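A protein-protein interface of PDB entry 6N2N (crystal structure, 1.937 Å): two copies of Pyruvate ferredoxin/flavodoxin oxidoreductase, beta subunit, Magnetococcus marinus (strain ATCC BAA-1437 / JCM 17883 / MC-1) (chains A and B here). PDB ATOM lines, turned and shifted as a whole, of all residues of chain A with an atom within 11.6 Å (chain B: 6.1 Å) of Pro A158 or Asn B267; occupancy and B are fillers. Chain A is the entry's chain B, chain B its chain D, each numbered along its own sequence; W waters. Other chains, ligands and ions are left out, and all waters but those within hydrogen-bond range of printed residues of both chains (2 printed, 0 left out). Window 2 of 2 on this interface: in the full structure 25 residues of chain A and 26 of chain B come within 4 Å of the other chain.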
ATOM      1  N   GLN A 139      -4.230  20.676  30.479  1.00  0.00           N
ATOM      2  CA  GLN A 139      -4.829  21.293  29.304  1.00  0.00           C
ATOM      3  C   GLN A 139      -4.407  20.519  28.061  1.00  0.00           C
ATOM      4  O   GLN A 139      -3.376  19.842  28.047  1.00  0.00           O
ATOM      5  CB  GLN A 139      -4.428  22.769  29.166  1.00  0.00           C
ATOM      6  CG  GLN A 139      -4.709  23.620  30.395  1.00  0.00           C
ATOM      7  CD  GLN A 139      -3.651  23.441  31.471  1.00  0.00           C
ATOM      8  OE1 GLN A 139      -2.475  23.234  31.165  1.00  0.00           O
ATOM      9  NE2 GLN A 139      -4.067  23.488  32.736  1.00  0.00           N
ATOM     10  N   TYR A 140      -5.217  20.622  27.010  1.00  0.00           N
ATOM     11  CA  TYR A 140      -4.931  19.834  25.820  1.00  0.00           C
ATOM     12  C   TYR A 140      -3.757  20.431  25.046  1.00  0.00           C
ATOM     13  O   TYR A 140      -3.382  21.592  25.230  1.00  0.00           O
ATOM     14  CB  TYR A 140      -6.174  19.703  24.937  1.00  0.00           C
ATOM     15  CG  TYR A 140      -6.504  20.889  24.055  1.00  0.00           C
ATOM     16  CD1 TYR A 140      -6.368  22.200  24.508  1.00  0.00           C
ATOM     17  CD2 TYR A 140      -6.967  20.689  22.760  1.00  0.00           C
ATOM     18  CE1 TYR A 140      -6.680  23.280  23.676  1.00  0.00           C
ATOM     19  CE2 TYR A 140      -7.279  21.747  21.942  1.00  0.00           C
ATOM     20  CZ  TYR A 140      -7.136  23.037  22.398  1.00  0.00           C
ATOM     21  OH  TYR A 140      -7.458  24.081  21.555  1.00  0.00           O
ATOM     22  N   SER A 141      -3.177  19.609  24.181  1.00  0.00           N
ATOM     23  CA  SER A 141      -1.950  19.887  23.451  1.00  0.00           C
ATOM     24  C   SER A 141      -2.185  19.722  21.959  1.00  0.00           C
ATOM     25  O   SER A 141      -3.255  19.271  21.535  1.00  0.00           O
ATOM     26  CB  SER A 141      -0.839  18.936  23.929  1.00  0.00           C
ATOM     27  OG  SER A 141      -0.880  17.714  23.213  1.00  0.00           O
ATOM     28  N   PRO A 142      -1.204  20.089  21.124  1.00  0.00           N
ATOM     29  CA  PRO A 142      -1.356  19.877  19.671  1.00  0.00           C
ATOM     30  C   PRO A 142      -1.470  18.415  19.249  1.00  0.00           C
ATOM     31  O   PRO A 142      -1.812  18.161  18.088  1.00  0.00           O
ATOM     32  CB  PRO A 142      -0.086  20.514  19.087  1.00  0.00           C
ATOM     33  CG  PRO A 142       0.331  21.522  20.095  1.00  0.00           C
ATOM     34  CD  PRO A 142      -0.017  20.913  21.429  1.00  0.00           C
ATOM     35  N   THR A 143      -1.194  17.454  20.131  1.00  0.00           N
ATOM     36  CA  THR A 143      -1.362  16.043  19.805  1.00  0.00           C
ATOM     37  C   THR A 143      -2.585  15.423  20.464  1.00  0.00           C
ATOM     38  O   THR A 143      -2.838  14.228  20.266  1.00  0.00           O
ATOM     39  CB  THR A 143      -0.111  15.238  20.189  1.00  0.00           C
ATOM     40  OG1 THR A 143       0.098  15.302  21.605  1.00  0.00           O
ATOM     41  CG2 THR A 143       1.119  15.771  19.472  1.00  0.00           C
ATOM     42  N   SER A 144      -3.346  16.198  21.236  1.00  0.00           N
ATOM     43  CA  SER A 144      -4.553  15.683  21.870  1.00  0.00           C
ATOM     44  C   SER A 144      -5.587  15.293  20.820  1.00  0.00           C
ATOM     45  O   SER A 144      -5.731  15.955  19.788  1.00  0.00           O
ATOM     46  CB  SER A 144      -5.155  16.734  22.810  1.00  0.00           C
ATOM     47  OG  SER A 144      -4.252  17.126  23.826  1.00  0.00           O
ATOM     48  N   ARG A 145      -6.332  14.219  21.102  1.00  0.00           N
ATOM     49  CA  ARG A 145      -7.438  13.847  20.238  1.00  0.00           C
ATOM     50  C   ARG A 145      -8.651  14.737  20.516  1.00  0.00           C
ATOM     51  O   ARG A 145      -8.865  15.166  21.654  1.00  0.00           O
ATOM     52  CB  ARG A 145      -7.800  12.377  20.445  1.00  0.00           C
ATOM     53  CG  ARG A 145      -6.726  11.399  19.956  1.00  0.00           C
ATOM     54  CD  ARG A 145      -7.184   9.950  20.092  1.00  0.00           C
ATOM     55  NE  ARG A 145      -6.951   9.402  21.426  1.00  0.00           N
ATOM     56  CZ  ARG A 145      -7.667   8.417  21.964  1.00  0.00           C
ATOM     57  NH1 ARG A 145      -8.677   7.884  21.291  1.00  0.00           N
ATOM     58  NH2 ARG A 145      -7.379   7.968  23.179  1.00  0.00           N
ATOM     59  N   PRO A 146      -9.457  15.030  19.491  1.00  0.00           N
ATOM     60  CA  PRO A 146     -10.541  16.012  19.669  1.00  0.00           C
ATOM     61  C   PRO A 146     -11.615  15.579  20.652  1.00  0.00           C
ATOM     62  O   PRO A 146     -12.261  16.439  21.269  1.00  0.00           O
ATOM     63  CB  PRO A 146     -11.114  16.161  18.250  1.00  0.00           C
ATOM     64  CG  PRO A 146     -10.071  15.622  17.345  1.00  0.00           C
ATOM     65  CD  PRO A 146      -9.380  14.540  18.107  1.00  0.00           C
ATOM     66  N   GLU A 147     -11.839  14.274  20.812  1.00  0.00           N
ATOM     67  CA  GLU A 147     -12.847  13.796  21.749  1.00  0.00           C
ATOM     68  C   GLU A 147     -12.433  13.970  23.205  1.00  0.00           C
ATOM     69  O   GLU A 147     -13.289  13.852  24.089  1.00  0.00           O
ATOM     70  CB  GLU A 147     -13.160  12.321  21.479  1.00  0.00           C
ATOM     71  CG  GLU A 147     -11.961  11.389  21.586  1.00  0.00           C
ATOM     72  CD  GLU A 147     -11.281  11.132  20.246  1.00  0.00           C
ATOM     73  OE1 GLU A 147     -11.263  12.038  19.385  1.00  0.00           O
ATOM     74  OE2 GLU A 147     -10.762  10.011  20.057  1.00  0.00           O
ATOM     75  N   MET A 148     -11.155  14.229  23.476  1.00  0.00           N
ATOM     76  CA  MET A 148     -10.709  14.444  24.846  1.00  0.00           C
ATOM     77  C   MET A 148     -11.299  15.737  25.390  1.00  0.00           C
ATOM     78  O   MET A 148     -11.392  16.743  24.682  1.00  0.00           O
ATOM     79  CB  MET A 148      -9.178  14.498  24.912  1.00  0.00           C
ATOM     80  CG  MET A 148      -8.594  14.431  26.329  1.00  0.00           C
ATOM     81  SD  MET A 148      -6.785  14.359  26.419  1.00  0.00           S
ATOM     82  CE  MET A 148      -6.343  16.091  26.249  1.00  0.00           C
ATOM     83  N   THR A 149     -11.724  15.699  26.649  1.00  0.00           N
ATOM     84  CA  THR A 149     -12.070  16.906  27.381  1.00  0.00           C
ATOM     85  C   THR A 149     -10.945  17.222  28.356  1.00  0.00           C
ATOM     86  O   THR A 149     -10.373  16.317  28.973  1.00  0.00           O
ATOM     87  CB  THR A 149     -13.402  16.757  28.126  1.00  0.00           C
ATOM     88  OG1 THR A 149     -13.326  15.665  29.048  1.00  0.00           O
ATOM     89  CG2 THR A 149     -14.555  16.517  27.148  1.00  0.00           C
ATOM     90  N   ALA A 150     -10.629  18.506  28.491  1.00  0.00           N
ATOM     91  CA  ALA A 150      -9.549  18.943  29.364  1.00  0.00           C
ATOM     92  C   ALA A 150      -9.939  20.289  29.961  1.00  0.00           C
ATOM     93  O   ALA A 150     -11.022  20.811  29.693  1.00  0.00           O
ATOM     94  CB  ALA A 150      -8.222  19.003  28.603  1.00  0.00           C
ATOM     95  N   TYR A 151      -9.042  20.869  30.764  1.00  0.00           N
ATOM     96  CA  TYR A 151      -9.471  21.941  31.663  1.00  0.00           C
ATOM     97  C   TYR A 151      -9.723  23.273  30.964  1.00  0.00           C
ATOM     98  O   TYR A 151     -10.473  24.096  31.500  1.00  0.00           O
ATOM     99  CB  TYR A 151      -8.461  22.095  32.797  1.00  0.00           C
ATOM    100  CG  TYR A 151      -8.759  21.091  33.882  1.00  0.00           C
ATOM    101  CD1 TYR A 151     -10.070  20.863  34.289  1.00  0.00           C
ATOM    102  CD2 TYR A 151      -7.754  20.321  34.452  1.00  0.00           C
ATOM    103  CE1 TYR A 151     -10.364  19.930  35.258  1.00  0.00           C
ATOM    104  CE2 TYR A 151      -8.041  19.382  35.421  1.00  0.00           C
ATOM    105  CZ  TYR A 151      -9.346  19.192  35.821  1.00  0.00           C
ATOM    106  OH  TYR A 151      -9.634  18.258  36.789  1.00  0.00           O
ATOM    107  N   THR A 152      -9.145  23.511  29.789  1.00  0.00           N
ATOM    108  CA  THR A 152      -9.554  24.652  28.975  1.00  0.00           C
ATOM    109  C   THR A 152     -10.455  24.237  27.822  1.00  0.00           C
ATOM    110  O   THR A 152     -10.937  25.101  27.081  1.00  0.00           O
ATOM    111  CB  THR A 152      -8.338  25.397  28.423  1.00  0.00           C
ATOM    112  OG1 THR A 152      -7.514  24.486  27.686  1.00  0.00           O
ATOM    113  CG2 THR A 152      -7.523  26.001  29.558  1.00  0.00           C
ATOM    114  N   THR A 153     -10.689  22.939  27.659  1.00  0.00           N
ATOM    115  CA  THR A 153     -11.584  22.409  26.631  1.00  0.00           C
ATOM    116  C   THR A 153     -12.601  21.471  27.276  1.00  0.00           C
ATOM    117  O   THR A 153     -12.645  20.274  26.970  1.00  0.00           O
ATOM    118  CB  THR A 153     -10.783  21.688  25.549  1.00  0.00           C
ATOM    119  OG1 THR A 153      -9.806  20.845  26.168  1.00  0.00           O
ATOM    120  CG2 THR A 153     -10.075  22.696  24.637  1.00  0.00           C
ATOM    121  N   PRO A 154     -13.438  21.983  28.187  1.00  0.00           N
ATOM    122  CA  PRO A 154     -14.428  21.111  28.835  1.00  0.00           C
ATOM    123  C   PRO A 154     -15.476  20.576  27.873  1.00  0.00           C
ATOM    124  O   PRO A 154     -16.197  19.636  28.232  1.00  0.00           O
ATOM    125  CB  PRO A 154     -15.060  22.026  29.888  1.00  0.00           C
ATOM    126  CG  PRO A 154     -14.959  23.395  29.284  1.00  0.00           C
ATOM    127  CD  PRO A 154     -13.658  23.405  28.519  1.00  0.00           C
ATOM    128  N   TYR A 155     -15.577  21.134  26.665  1.00  0.00           N
ATOM    129  CA  TYR A 155     -16.544  20.680  25.675  1.00  0.00           C
ATOM    130  C   TYR A 155     -15.872  20.011  24.478  1.00  0.00           C
ATOM    131  O   TYR A 155     -16.452  19.974  23.387  1.00  0.00           O
ATOM    132  CB  TYR A 155     -17.425  21.853  25.236  1.00  0.00           C
ATOM    133  CG  TYR A 155     -17.986  22.633  26.409  1.00  0.00           C
ATOM    134  CD1 TYR A 155     -18.852  22.028  27.316  1.00  0.00           C
ATOM    135  CD2 TYR A 155     -17.644  23.965  26.621  1.00  0.00           C
ATOM    136  CE1 TYR A 155     -19.365  22.724  28.399  1.00  0.00           C
ATOM    137  CE2 TYR A 155     -18.158  24.676  27.702  1.00  0.00           C
ATOM    138  CZ  TYR A 155     -19.020  24.046  28.590  1.00  0.00           C
ATOM    139  OH  TYR A 155     -19.537  24.738  29.671  1.00  0.00           O
ATOM    140  N   GLY A 156     -14.668  19.481  24.663  1.00  0.00           N
ATOM    141  CA  GLY A 156     -13.921  18.848  23.595  1.00  0.00           C
ATOM    142  C   GLY A 156     -13.005  19.822  22.869  1.00  0.00           C
ATOM    143  O   GLY A 156     -13.157  21.042  22.937  1.00  0.00           O
ATOM    144  N   GLY A 157     -12.038  19.260  22.144  1.00  0.00           N
ATOM    145  CA  GLY A 157     -11.103  20.057  21.380  1.00  0.00           C
ATOM    146  C   GLY A 157     -11.669  20.473  20.036  1.00  0.00           C
ATOM    147  O   GLY A 157     -12.141  19.643  19.255  1.00  0.00           O
ATOM    148  N   PRO A 158     -11.652  21.775  19.746  1.00  0.00           N
ATOM    149  CA  PRO A 158     -12.283  22.254  18.510  1.00  0.00           C
ATOM    150  C   PRO A 158     -11.373  22.187  17.292  1.00  0.00           C
ATOM    151  O   PRO A 158     -11.557  22.961  16.344  1.00  0.00           O
ATOM    152  CB  PRO A 158     -12.650  23.701  18.855  1.00  0.00           C
ATOM    153  CG  PRO A 158     -11.595  24.116  19.820  1.00  0.00           C
ATOM    154  CD  PRO A 158     -11.286  22.887  20.643  1.00  0.00           C
ATOM    155  N   GLU A 159     -10.406  21.271  17.295  1.00  0.00           N
ATOM    156  CA  GLU A 159      -9.510  21.104  16.156  1.00  0.00           C
ATOM    157  C   GLU A 159      -8.892  19.712  16.208  1.00  0.00           C
ATOM    158  O   GLU A 159      -8.934  19.027  17.234  1.00  0.00           O
ATOM    159  CB  GLU A 159      -8.417  22.178  16.135  1.00  0.00           C
ATOM    160  CG  GLU A 159      -7.434  22.072  17.295  1.00  0.00           C
ATOM    161  CD  GLU A 159      -7.560  23.213  18.295  1.00  0.00           C
ATOM    162  OE1 GLU A 159      -6.767  23.239  19.257  1.00  0.00           O
ATOM    163  OE2 GLU A 159      -8.438  24.089  18.125  1.00  0.00           O
ATOM    164  N   ASN A 160      -8.299  19.314  15.080  1.00  0.00           N
ATOM    165  CA  ASN A 160      -7.581  18.059  14.932  1.00  0.00           C
ATOM    166  C   ASN A 160      -6.147  18.189  15.434  1.00  0.00           C
ATOM    167  O   ASN A 160      -5.590  19.289  15.474  1.00  0.00           O
ATOM    168  CB  ASN A 160      -7.563  17.628  13.467  1.00  0.00           C
ATOM    169  CG  ASN A 160      -8.938  17.256  12.946  1.00  0.00           C
ATOM    170  OD1 ASN A 160      -9.762  16.698  13.669  1.00  0.00           O
ATOM    171  ND2 ASN A 160      -9.191  17.570  11.680  1.00  0.00           N
ATOM    172  N   PRO A 161      -5.532  17.079  15.828  1.00  0.00           N
ATOM    173  CA  PRO A 161      -4.128  17.111  16.242  1.00  0.00           C
ATOM    174  C   PRO A 161      -3.176  17.108  15.054  1.00  0.00           C
ATOM    175  O   PRO A 161      -3.533  16.752  13.930  1.00  0.00           O
ATOM    176  CB  PRO A 161      -3.977  15.823  17.059  1.00  0.00           C
ATOM    177  CG  PRO A 161      -4.989  14.905  16.461  1.00  0.00           C
ATOM    178  CD  PRO A 161      -6.154  15.768  16.093  1.00  0.00           C
ATOM    179  N   MET A 162      -1.933  17.484  15.333  1.00  0.00           N
ATOM    180  CA  MET A 162      -0.886  17.464  14.323  1.00  0.00           C
ATOM    181  C   MET A 162      -0.119  16.144  14.352  1.00  0.00           C
ATOM    182  O   MET A 162      -0.324  15.284  15.213  1.00  0.00           O
ATOM    183  CB  MET A 162       0.071  18.650  14.498  1.00  0.00           C
ATOM    184  CG  MET A 162       0.466  18.974  15.927  1.00  0.00           C
ATOM    185  SD  MET A 162       1.915  18.097  16.546  1.00  0.00           S
ATOM    186  CE  MET A 162       3.191  18.497  15.355  1.00  0.00           C
ATOM    187  N   LYS B 119      -5.980  24.190  12.558  1.00  0.00           N
ATOM    188  CA  LYS B 119      -7.318  24.546  13.014  1.00  0.00           C
ATOM    189  C   LYS B 119      -8.264  24.906  11.879  1.00  0.00           C
ATOM    190  O   LYS B 119      -9.446  25.150  12.141  1.00  0.00           O
ATOM    191  CB  LYS B 119      -7.233  25.705  14.005  1.00  0.00           C
ATOM    192  CG  LYS B 119      -6.445  25.342  15.261  1.00  0.00           C
ATOM    193  CD  LYS B 119      -6.302  26.514  16.203  1.00  0.00           C
ATOM    194  CE  LYS B 119      -5.471  26.124  17.425  1.00  0.00           C
ATOM    195  NZ  LYS B 119      -5.483  27.199  18.439  1.00  0.00           N
ATOM    196  N   PRO B 262     -14.517  20.851   8.780  1.00  0.00           N
ATOM    197  CA  PRO B 262     -15.036  21.921   9.644  1.00  0.00           C
ATOM    198  C   PRO B 262     -13.984  22.993   9.901  1.00  0.00           C
ATOM    199  O   PRO B 262     -12.795  22.701  10.033  1.00  0.00           O
ATOM    200  CB  PRO B 262     -15.419  21.183  10.931  1.00  0.00           C
ATOM    201  CG  PRO B 262     -15.664  19.775  10.498  1.00  0.00           C
ATOM    202  CD  PRO B 262     -14.693  19.518   9.384  1.00  0.00           C
ATOM    203  N   THR B 263     -14.429  24.245   9.956  1.00  0.00           N
ATOM    204  CA  THR B 263     -13.514  25.334  10.254  1.00  0.00           C
ATOM    205  C   THR B 263     -13.504  25.610  11.750  1.00  0.00           C
ATOM    206  O   THR B 263     -14.382  25.171  12.493  1.00  0.00           O
ATOM    207  CB  THR B 263     -13.896  26.608   9.500  1.00  0.00           C
ATOM    208  OG1 THR B 263     -15.075  27.180  10.085  1.00  0.00           O
ATOM    209  CG2 THR B 263     -14.142  26.316   8.018  1.00  0.00           C
ATOM    210  N   LEU B 264     -12.502  26.376  12.189  1.00  0.00           N
ATOM    211  CA  LEU B 264     -12.391  26.696  13.607  1.00  0.00           C
ATOM    212  C   LEU B 264     -13.644  27.410  14.102  1.00  0.00           C
ATOM    213  O   LEU B 264     -14.191  27.061  15.152  1.00  0.00           O
ATOM    214  CB  LEU B 264     -11.141  27.539  13.870  1.00  0.00           C
ATOM    215  CG  LEU B 264     -10.911  27.935  15.335  1.00  0.00           C
ATOM    216  CD1 LEU B 264     -10.825  26.698  16.227  1.00  0.00           C
ATOM    217  CD2 LEU B 264      -9.652  28.788  15.474  1.00  0.00           C
ATOM    218  N   ASP B 265     -14.129  28.402  13.350  1.00  0.00           N
ATOM    219  CA  ASP B 265     -15.316  29.117  13.809  1.00  0.00           C
ATOM    220  C   ASP B 265     -16.537  28.204  13.827  1.00  0.00           C
ATOM    221  O   ASP B 265     -17.428  28.378  14.670  1.00  0.00           O
ATOM    222  CB  ASP B 265     -15.556  30.375  12.961  1.00  0.00           C
ATOM    223  CG  ASP B 265     -16.134  30.080  11.572  1.00  0.00           C
ATOM    224  OD1 ASP B 265     -17.343  29.771  11.473  1.00  0.00           O
ATOM    225  OD2 ASP B 265     -15.392  30.216  10.572  1.00  0.00           O
ATOM    226  N   GLN B 266     -16.578  27.203  12.942  1.00  0.00           N
ATOM    227  CA  GLN B 266     -17.677  26.243  12.967  1.00  0.00           C
ATOM    228  C   GLN B 266     -17.625  25.359  14.211  1.00  0.00           C
ATOM    229  O   GLN B 266     -18.661  25.092  14.832  1.00  0.00           O
ATOM    230  CB  GLN B 266     -17.656  25.392  11.699  1.00  0.00           C
ATOM    231  CG  GLN B 266     -18.154  26.132  10.473  1.00  0.00           C
ATOM    232  CD  GLN B 266     -17.987  25.334   9.200  1.00  0.00           C
ATOM    233  OE1 GLN B 266     -17.220  24.369   9.150  1.00  0.00           O
ATOM    234  NE2 GLN B 266     -18.708  25.731   8.157  1.00  0.00           N
ATOM    235  N   ASN B 267     -16.434  24.891  14.589  1.00  0.00           N
ATOM    236  CA  ASN B 267     -16.322  24.053  15.781  1.00  0.00           C
ATOM    237  C   ASN B 267     -16.572  24.856  17.053  1.00  0.00           C
ATOM    238  O   ASN B 267     -17.194  24.356  18.000  1.00  0.00           O
ATOM    239  CB  ASN B 267     -14.955  23.373  15.816  1.00  0.00           C
ATOM    240  CG  ASN B 267     -14.853  22.230  14.819  1.00  0.00           C
ATOM    241  OD1 ASN B 267     -15.842  21.571  14.512  1.00  0.00           O
ATOM    242  ND2 ASN B 267     -13.655  21.992  14.311  1.00  0.00           N
ATOM    243  N   LEU B 268     -16.102  26.103  17.097  1.00  0.00           N
ATOM    244  CA  LEU B 268     -16.416  26.954  18.238  1.00  0.00           C
ATOM    245  C   LEU B 268     -17.918  27.194  18.340  1.00  0.00           C
ATOM    246  O   LEU B 268     -18.487  27.181  19.440  1.00  0.00           O
ATOM    247  CB  LEU B 268     -15.657  28.277  18.126  1.00  0.00           C
ATOM    248  CG  LEU B 268     -14.128  28.184  18.214  1.00  0.00           C
ATOM    249  CD1 LEU B 268     -13.490  29.547  18.000  1.00  0.00           C
ATOM    250  CD2 LEU B 268     -13.699  27.604  19.557  1.00  0.00           C
ATOM    251  N   ALA B 269     -18.584  27.386  17.198  1.00  0.00           N
ATOM    252  CA  ALA B 269     -20.030  27.589  17.205  1.00  0.00           C
ATOM    253  C   ALA B 269     -20.768  26.345  17.689  1.00  0.00           C
ATOM    254  O   ALA B 269     -21.779  26.458  18.390  1.00  0.00           O
ATOM    255  CB  ALA B 269     -20.518  27.999  15.816  1.00  0.00           C
ATOM    256  N   LYS B 270     -20.305  25.154  17.297  1.00  0.00           N
ATOM    257  CA  LYS B 270     -20.921  23.917  17.784  1.00  0.00           C
ATOM    258  C   LYS B 270     -20.910  23.849  19.306  1.00  0.00           C
ATOM    259  O   LYS B 270     -21.884  23.402  19.923  1.00  0.00           O
ATOM    260  CB  LYS B 270     -20.206  22.698  17.203  1.00  0.00           C
ATOM    261  CG  LYS B 270     -20.413  22.514  15.714  1.00  0.00           C
ATOM    262  CD  LYS B 270     -19.577  21.371  15.160  1.00  0.00           C
ATOM    263  CE  LYS B 270     -19.600  21.379  13.636  1.00  0.00           C
ATOM    264  NZ  LYS B 270     -18.672  20.369  13.055  1.00  0.00           N
ATOM    265  N   ILE B 271     -19.815  24.293  19.925  1.00  0.00           N
ATOM    266  CA  ILE B 271     -19.712  24.297  21.381  1.00  0.00           C
ATOM    267  C   ILE B 271     -20.799  25.178  21.987  1.00  0.00           C
ATOM    268  O   ILE B 271     -21.479  24.786  22.942  1.00  0.00           O
ATOM    269  CB  ILE B 271     -18.302  24.746  21.807  1.00  0.00           C
ATOM    270  CG1 ILE B 271     -17.271  23.690  21.400  1.00  0.00           C
ATOM    271  CG2 ILE B 271     -18.248  25.040  23.298  1.00  0.00           C
ATOM    272  CD1 ILE B 271     -15.828  24.094  21.665  1.00  0.00           C
ATOM    273  N   ARG B 272     -20.980  26.381  21.438  1.00  0.00           N
ATOM    274  CA  ARG B 272     -22.024  27.274  21.937  1.00  0.00           C
ATOM    275  C   ARG B 272     -23.414  26.697  21.688  1.00  0.00           C
ATOM    276  O   ARG B 272     -24.297  26.798  22.550  1.00  0.00           O
ATOM    277  CB  ARG B 272     -21.887  28.655  21.290  1.00  0.00           C
ATOM    278  CG  ARG B 272     -20.574  29.361  21.602  1.00  0.00           C
ATOM    279  CD  ARG B 272     -20.605  30.841  21.223  1.00  0.00           C
ATOM    280  NE  ARG B 272     -21.269  31.092  19.941  1.00  0.00           N
ATOM    281  CZ  ARG B 272     -20.654  31.129  18.761  1.00  0.00           C
ATOM    282  NH1 ARG B 272     -19.346  30.932  18.671  1.00  0.00           N
ATOM    283  NH2 ARG B 272     -21.353  31.365  17.663  1.00  0.00           N
HETATM  284  O   HOH W   1     -10.775  23.347  13.854  1.00  0.00           O
HETATM  285  O   HOH W   2      -8.049  26.757  19.183  1.00  0.00           O
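The side-chain carboxylate (OE1) of Glu A159 is in hydrogen-bond range of the side-chain hydroxyl (OH) of Tyr A140. The backbone NH (N) of Leu B264 sits at hydrogen-bond distance from the backbone carbonyl oxygen (O) of Lys B119 (3.3 Å). The side-chain amide oxygen (OD1) of Asn B267 lies within hydrogen-bond range of the side-chain amino group (NZ) of Lys B270.
Printed residues of chain B that touch a printed residue of chain A: Lys B119, Leu B264, Asn B267 and Ile B271. Printed residues of chain A that touch a printed residue of chain B: Tyr A155, Pro A158 and Glu A159. Hydrophobic or aromatic side chains of chain A that line the printed part of chain B: Tyr A155 and Pro A158. Among the printed residues, 4 pairs touch across the chains. Among the printed residues, no Asp or Glu carboxylate lies within 4 Å of a Lys or Arg side-chain nitrogen of the other chain.
Among the printed residues, merely in contact across the chains: Tyr A155 with Ile B271, Glu A159 with Lys B119 and Pro A158 with Leu B264.
The backbone carbonyl oxygen (O) of Pro A158 lies within hydrogen-bond range of the side-chain amide nitrogen (ND2) of Asn B267 (3.1 Å).
No position is printed for both chains. Of the 4 pairs that touch across the chains among the printed residues, none has its exchanged pair printed and touching as well.
Water W1 lies within hydrogen-bond range of the backbone carbonyl oxygen of Pro A158 (2.6 Å), the backbone carbonyl oxygen of Lys B119 (2.8 Å) and the side-chain amide nitrogen of Asn B267 (3.2 Å). Water W2 bridges NZ of Lys B119 and OE2 of Glu A159.
Of chain B, only Leu B264 and Asn B267 come within 4 Å of Pro A158. Asn B267 touches just one residue of chain A: Pro A158 (3.1 Å). No residue of chain A comes within 4 Å of Pro B262. Thr B263 touches none of the printed residues of chain A. Asp B265 touches none of the printed residues of chain A. Gln B266 touches none of the printed residues of chain A. No residue of chain A comes within 4 Å of Leu B268. No residue of chain A comes within 4 Å of Ala B269. No residue of chain A comes within 4 Å of Lys B270. Ile B271 touches just one residue of chain A: Tyr A155. Of the printed residues of chain B, Glu A159 touches Lys B119 (3.7 Å). Of the printed residues of chain A, Leu B264 touches Pro A158. Of the printed residues of chain B, Tyr A155 touches Ile B271. Met A148 touches none of the printed residues of chain B. The nearest residue of chain B that does not touch Pro A158 is Leu B268 (4.1 Å).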
